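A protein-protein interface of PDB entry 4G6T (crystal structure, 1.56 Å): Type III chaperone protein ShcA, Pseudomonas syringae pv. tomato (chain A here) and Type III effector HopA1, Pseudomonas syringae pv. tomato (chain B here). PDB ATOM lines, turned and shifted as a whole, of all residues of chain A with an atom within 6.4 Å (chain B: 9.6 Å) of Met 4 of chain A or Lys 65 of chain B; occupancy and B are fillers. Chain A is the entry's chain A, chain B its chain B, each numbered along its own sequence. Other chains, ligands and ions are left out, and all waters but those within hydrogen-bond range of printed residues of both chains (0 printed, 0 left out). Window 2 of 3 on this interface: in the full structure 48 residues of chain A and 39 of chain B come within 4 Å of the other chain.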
ATOM      1  N   VAL A   2     -13.143 -13.999 -23.323  1.00  0.00           N
ATOM      2  CA  VAL A   2     -12.640 -13.358 -22.137  1.00  0.00           C
ATOM      3  C   VAL A   2     -12.544 -11.840 -22.304  1.00  0.00           C
ATOM      4  O   VAL A   2     -11.909 -11.302 -23.237  1.00  0.00           O
ATOM      5  CB  VAL A   2     -11.245 -13.883 -21.837  1.00  0.00           C
ATOM      6  CG1 VAL A   2     -10.654 -13.126 -20.655  1.00  0.00           C
ATOM      7  CG2 VAL A   2     -11.262 -15.401 -21.633  1.00  0.00           C
ATOM      8  N   ASP A   3     -13.125 -11.146 -21.336  1.00  0.00           N
ATOM      9  CA  ASP A   3     -13.131  -9.716 -21.287  1.00  0.00           C
ATOM     10  C   ASP A   3     -11.791  -9.211 -20.745  1.00  0.00           C
ATOM     11  O   ASP A   3     -11.593  -9.057 -19.541  1.00  0.00           O
ATOM     12  CB  ASP A   3     -14.300  -9.270 -20.409  1.00  0.00           C
ATOM     13  CG  ASP A   3     -14.387  -7.781 -20.260  1.00  0.00           C
ATOM     14  OD1 ASP A   3     -13.455  -7.085 -20.680  1.00  0.00           O
ATOM     15  OD2 ASP A   3     -15.415  -7.304 -19.713  1.00  0.00           O
ATOM     16  N   MET A   4     -10.859  -8.919 -21.641  1.00  0.00           N
ATOM     17  CA  MET A   4      -9.503  -8.545 -21.233  1.00  0.00           C
ATOM     18  C   MET A   4      -9.399  -7.308 -20.349  1.00  0.00           C
ATOM     19  O   MET A   4      -8.423  -7.119 -19.635  1.00  0.00           O
ATOM     20  CB  MET A   4      -8.605  -8.396 -22.466  1.00  0.00           C
ATOM     21  CG  MET A   4      -8.624  -9.678 -23.293  1.00  0.00           C
ATOM     22  SD  MET A   4      -8.036 -11.181 -22.506  1.00  0.00           S
ATOM     23  CE  MET A   4      -6.229 -11.027 -22.566  1.00  0.00           C
ATOM     24  N   SER A   5     -10.417  -6.442 -20.362  1.00  0.00           N
ATOM     25  CA  SER A   5     -10.420  -5.295 -19.477  1.00  0.00           C
ATOM     26  C   SER A   5     -10.416  -5.678 -18.017  1.00  0.00           C
ATOM     27  O   SER A   5      -9.961  -4.883 -17.203  1.00  0.00           O
ATOM     28  CB  SER A   5     -11.615  -4.360 -19.777  1.00  0.00           C
ATOM     29  OG  SER A   5     -12.866  -4.941 -19.489  1.00  0.00           O
ATOM     30  N   ASN A   6     -10.880  -6.885 -17.747  1.00  0.00           N
ATOM     31  CA  ASN A   6     -10.884  -7.408 -16.368  1.00  0.00           C
ATOM     32  C   ASN A   6      -9.459  -7.666 -15.854  1.00  0.00           C
ATOM     33  O   ASN A   6      -9.282  -7.895 -14.635  1.00  0.00           O
ATOM     34  CB  ASN A   6     -11.761  -8.595 -16.190  1.00  0.00           C
ATOM     35  CG  ASN A   6     -13.236  -8.223 -16.173  1.00  0.00           C
ATOM     36  OD1 ASN A   6     -13.557  -7.083 -15.761  1.00  0.00           O
ATOM     37  ND2 ASN A   6     -14.099  -9.129 -16.578  1.00  0.00           N
ATOM     38  N   LEU A   7      -8.435  -7.606 -16.714  1.00  0.00           N
ATOM     39  CA  LEU A   7      -7.053  -7.694 -16.210  1.00  0.00           C
ATOM     40  C   LEU A   7      -6.538  -6.402 -15.599  1.00  0.00           C
ATOM     41  O   LEU A   7      -5.423  -6.322 -15.179  1.00  0.00           O
ATOM     42  CB  LEU A   7      -6.090  -8.201 -17.284  1.00  0.00           C
ATOM     43  CG  LEU A   7      -6.155  -9.672 -17.585  1.00  0.00           C
ATOM     44  CD1 LEU A   7      -5.614  -9.914 -18.983  1.00  0.00           C
ATOM     45  CD2 LEU A   7      -5.444 -10.427 -16.456  1.00  0.00           C
ATOM     46  N   PHE A   8      -7.340  -5.326 -15.607  1.00  0.00           N
ATOM     47  CA  PHE A   8      -6.982  -4.058 -14.984  1.00  0.00           C
ATOM     48  C   PHE A   8      -6.491  -4.214 -13.526  1.00  0.00           C
ATOM     49  O   PHE A   8      -5.565  -3.567 -13.121  1.00  0.00           O
ATOM     50  CB  PHE A   8      -8.219  -3.163 -14.999  1.00  0.00           C
ATOM     51  CG  PHE A   8      -7.984  -1.759 -14.546  1.00  0.00           C
ATOM     52  CD1 PHE A   8      -7.561  -0.809 -15.459  1.00  0.00           C
ATOM     53  CD2 PHE A   8      -8.139  -1.402 -13.221  1.00  0.00           C
ATOM     54  CE1 PHE A   8      -7.352   0.523 -15.074  1.00  0.00           C
ATOM     55  CE2 PHE A   8      -7.906  -0.078 -12.809  1.00  0.00           C
ATOM     56  CZ  PHE A   8      -7.504   0.872 -13.741  1.00  0.00           C
ATOM     57  N   GLN B  57     -14.985 -18.236 -12.255  1.00  0.00           N
ATOM     58  CA  GLN B  57     -14.863 -18.594 -13.681  1.00  0.00           C
ATOM     59  C   GLN B  57     -14.100 -17.530 -14.450  1.00  0.00           C
ATOM     60  O   GLN B  57     -13.186 -17.856 -15.241  1.00  0.00           O
ATOM     61  CB  GLN B  57     -16.233 -18.889 -14.297  1.00  0.00           C
ATOM     62  CG  GLN B  57     -16.775 -20.220 -13.797  1.00  0.00           C
ATOM     63  CD  GLN B  57     -18.125 -20.564 -14.379  1.00  0.00           C
ATOM     64  OE1 GLN B  57     -18.328 -20.473 -15.595  1.00  0.00           O
ATOM     65  NE2 GLN B  57     -19.064 -20.968 -13.514  1.00  0.00           N
ATOM     66  N   ILE B  58     -14.415 -16.264 -14.168  1.00  0.00           N
ATOM     67  CA  ILE B  58     -13.727 -15.160 -14.805  1.00  0.00           C
ATOM     68  C   ILE B  58     -12.254 -15.147 -14.406  1.00  0.00           C
ATOM     69  O   ILE B  58     -11.379 -15.066 -15.251  1.00  0.00           O
ATOM     70  CB  ILE B  58     -14.401 -13.781 -14.501  1.00  0.00           C
ATOM     71  CG1 ILE B  58     -15.720 -13.629 -15.280  1.00  0.00           C
ATOM     72  CG2 ILE B  58     -13.473 -12.632 -14.840  1.00  0.00           C
ATOM     73  CD1 ILE B  58     -16.634 -12.543 -14.733  1.00  0.00           C
ATOM     74  N   ALA B  59     -11.955 -15.288 -13.110  1.00  0.00           N
ATOM     75  CA  ALA B  59     -10.584 -15.209 -12.618  1.00  0.00           C
ATOM     76  C   ALA B  59      -9.695 -16.292 -13.238  1.00  0.00           C
ATOM     77  O   ALA B  59      -8.552 -16.039 -13.578  1.00  0.00           O
ATOM     78  CB  ALA B  59     -10.560 -15.327 -11.080  1.00  0.00           C
ATOM     79  N   GLN B  60     -10.234 -17.486 -13.334  1.00  0.00           N
ATOM     80  CA  GLN B  60      -9.475 -18.610 -13.865  1.00  0.00           C
ATOM     81  C   GLN B  60      -9.174 -18.352 -15.331  1.00  0.00           C
ATOM     82  O   GLN B  60      -8.047 -18.589 -15.774  1.00  0.00           O
ATOM     83  CB  GLN B  60     -10.274 -19.906 -13.686  1.00  0.00           C
ATOM     84  CG  GLN B  60      -9.549 -21.150 -14.184  1.00  0.00           C
ATOM     85  CD  GLN B  60     -10.305 -22.428 -13.841  1.00  0.00           C
ATOM     86  OE1 GLN B  60     -11.245 -22.416 -13.041  1.00  0.00           O
ATOM     87  NE2 GLN B  60      -9.898 -23.538 -14.446  1.00  0.00           N
ATOM     88  N   ALA B  61     -10.155 -17.842 -16.070  1.00  0.00           N
ATOM     89  CA  ALA B  61      -9.913 -17.514 -17.482  1.00  0.00           C
ATOM     90  C   ALA B  61      -8.893 -16.422 -17.703  1.00  0.00           C
ATOM     91  O   ALA B  61      -8.118 -16.493 -18.625  1.00  0.00           O
ATOM     92  CB  ALA B  61     -11.187 -17.155 -18.216  1.00  0.00           C
ATOM     93  N   LEU B  62      -8.893 -15.383 -16.863  1.00  0.00           N
ATOM     94  CA  LEU B  62      -7.937 -14.317 -16.970  1.00  0.00           C
ATOM     95  C   LEU B  62      -6.527 -14.851 -16.698  1.00  0.00           C
ATOM     96  O   LEU B  62      -5.588 -14.497 -17.352  1.00  0.00           O
ATOM     97  CB  LEU B  62      -8.285 -13.185 -15.951  1.00  0.00           C
ATOM     98  CG  LEU B  62      -9.568 -12.401 -16.187  1.00  0.00           C
ATOM     99  CD1 LEU B  62      -9.790 -11.499 -14.963  1.00  0.00           C
ATOM    100  CD2 LEU B  62      -9.463 -11.653 -17.512  1.00  0.00           C
ATOM    101  N   ASN B  63      -6.399 -15.702 -15.694  1.00  0.00           N
ATOM    102  CA  ASN B  63      -5.101 -16.211 -15.337  1.00  0.00           C
ATOM    103  C   ASN B  63      -4.506 -17.087 -16.424  1.00  0.00           C
ATOM    104  O   ASN B  63      -3.282 -17.049 -16.637  1.00  0.00           O
ATOM    105  CB  ASN B  63      -5.166 -16.878 -13.969  1.00  0.00           C
ATOM    106  CG  ASN B  63      -5.208 -15.861 -12.847  1.00  0.00           C
ATOM    107  OD1 ASN B  63      -4.803 -14.728 -13.006  1.00  0.00           O
ATOM    108  ND2 ASN B  63      -5.693 -16.273 -11.708  1.00  0.00           N
ATOM    109  N   GLU B  64      -5.376 -17.797 -17.126  1.00  0.00           N
ATOM    110  CA  GLU B  64      -4.962 -18.599 -18.304  1.00  0.00           C
ATOM    111  C   GLU B  64      -4.440 -17.683 -19.413  1.00  0.00           C
ATOM    112  O   GLU B  64      -3.413 -17.977 -20.058  1.00  0.00           O
ATOM    113  CB  GLU B  64      -6.114 -19.437 -18.759  1.00  0.00           C
ATOM    114  CG  GLU B  64      -5.960 -20.155 -20.083  1.00  0.00           C
ATOM    115  CD  GLU B  64      -7.242 -20.895 -20.437  1.00  0.00           C
ATOM    116  OE1 GLU B  64      -8.107 -21.027 -19.530  1.00  0.00           O
ATOM    117  OE2 GLU B  64      -7.393 -21.324 -21.605  1.00  0.00           O
ATOM    118  N   LYS B  65      -5.123 -16.558 -19.637  1.00  0.00           N
ATOM    119  CA  LYS B  65      -4.654 -15.604 -20.628  1.00  0.00           C
ATOM    120  C   LYS B  65      -3.313 -15.015 -20.303  1.00  0.00           C
ATOM    121  O   LYS B  65      -2.510 -14.754 -21.203  1.00  0.00           O
ATOM    122  CB  LYS B  65      -5.675 -14.481 -20.941  1.00  0.00           C
ATOM    123  CG  LYS B  65      -6.941 -15.047 -21.559  1.00  0.00           C
ATOM    124  CD  LYS B  65      -6.712 -15.364 -23.036  1.00  0.00           C
ATOM    125  CE  LYS B  65      -7.878 -16.072 -23.700  1.00  0.00           C
ATOM    126  NZ  LYS B  65      -7.957 -17.491 -23.290  1.00  0.00           N
ATOM    127  N   VAL B  66      -3.078 -14.766 -19.016  1.00  0.00           N
ATOM    128  CA  VAL B  66      -1.813 -14.238 -18.540  1.00  0.00           C
ATOM    129  C   VAL B  66      -0.691 -15.256 -18.806  1.00  0.00           C
ATOM    130  O   VAL B  66       0.378 -14.896 -19.268  1.00  0.00           O
ATOM    131  CB  VAL B  66      -1.884 -13.887 -17.035  1.00  0.00           C
ATOM    132  CG1 VAL B  66      -0.510 -13.627 -16.430  1.00  0.00           C
ATOM    133  CG2 VAL B  66      -2.813 -12.687 -16.817  1.00  0.00           C
ATOM    134  N   ALA B  67      -0.997 -16.517 -18.528  1.00  0.00           N
ATOM    135  CA  ALA B  67      -0.030 -17.593 -18.786  1.00  0.00           C
ATOM    136  C   ALA B  67       0.291 -17.685 -20.262  1.00  0.00           C
ATOM    137  O   ALA B  67       1.445 -17.866 -20.649  1.00  0.00           O
ATOM    138  CB  ALA B  67      -0.581 -18.921 -18.261  1.00  0.00           C
ATOM    139  N   SER B  68      -0.719 -17.537 -21.110  1.00  0.00           N
ATOM    140  CA  SER B  68      -0.479 -17.511 -22.569  1.00  0.00           C
ATOM    141  C   SER B  68       0.413 -16.363 -23.039  1.00  0.00           C
ATOM    142  O   SER B  68       1.249 -16.519 -23.957  1.00  0.00           O
ATOM    143  CB  SER B  68      -1.804 -17.412 -23.300  1.00  0.00           C
ATOM    144  OG  SER B  68      -2.589 -18.534 -23.096  1.00  0.00           O
ATOM    145  N   ALA B  69       0.222 -15.173 -22.475  1.00  0.00           N
ATOM    146  CA  ALA B  69       1.019 -14.043 -22.904  1.00  0.00           C
ATOM    147  C   ALA B  69       2.481 -14.283 -22.552  1.00  0.00           C
ATOM    148  O   ALA B  69       3.368 -13.924 -23.301  1.00  0.00           O
ATOM    149  CB  ALA B  69       0.495 -12.769 -22.304  1.00  0.00           C
ATOM    150  N   ARG B  70       2.728 -14.933 -21.422  1.00  0.00           N
ATOM    151  CA  ARG B  70       4.105 -15.255 -21.031  1.00  0.00           C
ATOM    152  C   ARG B  70       4.768 -16.196 -22.046  1.00  0.00           C
ATOM    153  O   ARG B  70       5.931 -16.003 -22.390  1.00  0.00           O
ATOM    154  CB  ARG B  70       4.114 -15.935 -19.678  1.00  0.00           C
ATOM    155  CG  ARG B  70       4.015 -14.939 -18.568  1.00  0.00           C
ATOM    156  CD  ARG B  70       3.651 -15.637 -17.287  1.00  0.00           C
ATOM    157  NE  ARG B  70       3.340 -14.638 -16.274  1.00  0.00           N
ATOM    158  CZ  ARG B  70       2.722 -14.900 -15.129  1.00  0.00           C
ATOM    159  NH1 ARG B  70       2.363 -16.143 -14.813  1.00  0.00           N
ATOM    160  NH2 ARG B  70       2.492 -13.899 -14.293  1.00  0.00           N
ATOM    161  N   THR B  71       4.017 -17.186 -22.518  1.00  0.00           N
ATOM    162  CA  THR B  71       4.519 -18.102 -23.559  1.00  0.00           C
ATOM    163  C   THR B  71       4.927 -17.398 -24.870  1.00  0.00           C
ATOM    164  O   THR B  71       5.915 -17.776 -25.510  1.00  0.00           O
ATOM    165  CB  THR B  71       3.469 -19.162 -23.859  1.00  0.00           C
ATOM    166  OG1 THR B  71       3.221 -19.894 -22.655  1.00  0.00           O
ATOM    167  CG2 THR B  71       3.938 -20.128 -24.938  1.00  0.00           C
ATOM    168  N   VAL B  72       4.193 -16.356 -25.259  1.00  0.00           N
ATOM    169  CA  VAL B  72       4.552 -15.554 -26.437  1.00  0.00           C
ATOM    170  C   VAL B  72       5.974 -14.993 -26.316  1.00  0.00           C
ATOM    171  O   VAL B  72       6.731 -15.019 -27.281  1.00  0.00           O
ATOM    172  CB  VAL B  72       3.517 -14.416 -26.705  1.00  0.00           C
ATOM    173  CG1 VAL B  72       4.059 -13.355 -27.679  1.00  0.00           C
ATOM    174  CG2 VAL B  72       2.196 -15.021 -27.210  1.00  0.00           C
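Of the 7 printed residues of chain A, 5 touch a printed residue of chain B.
Hydrophobic or aromatic side chains of chain A that line the printed part of chain B: Val 2, Met 4 and Leu 7.
Along chain A the printed residues that touch a printed residue of chain B span positions 2 to 7.
Of the 16 printed residues of chain B, 5 touch a printed residue of chain A.
Along chain B the printed residues that touch a printed residue of chain A span positions 58 to 66.
OD1 of Asp 3 of chain A sits at hydrogen-bond distance from OG of Ser 5 of chain A, at 2.5 Å.
Printed residues of chain B within 4 Å of Val 2 of chain A: Ala 61 and Leu 62.
Printed residues of chain B within 4 Å of Asp 3 of chain A: Leu 62.
Of chain B, only Lys 65 comes within 4 Å of Met 4 of chain A.
No residue of chain B comes within 4 Å of Ser 5 of chain A.
Leu 7 of chain A touches two residues of chain B.
Ala 59 of chain B touches none of the printed residues of chain A.
Printed residues of chain A within 4 Å of Ala 61 of chain B: Val 2 (3.8 Å).
Printed residues of chain A within 4 Å of Leu 62 of chain B: Val 2, Asp 3, Asn 6 and Leu 7.
Lys 65 of chain B touches one residue of chain A.
The nearest residue of chain A that does not touch Lys 65 of chain B is Val 2 of chain A (4.02 Å).
The nearest printed residue of chain A that does not touch Leu 62 of chain B is Met 4 of chain A (4.8 Å).
Among the printed residues, pairs that only touch across the chains: Leu 7 of chain A with Val 66 of chain B (3.5 Å), Asn 6 of chain A with Leu 62 of chain B (3.7 Å), Val 2 of chain A with Leu 62 of chain B (3.7 Å), Val 2 of chain A with Ala 61 of chain B (3.8 Å), Leu 7 of chain A with Leu 62 of chain B (3.9 Å), Met 4 of chain A with Lys 65 of chain B (3.9 Å), Asp 3 of chain A with Leu 62 of chain B (3.9 Å) and Asn 6 of chain A with Ile 58 of chain B (3.96 Å).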
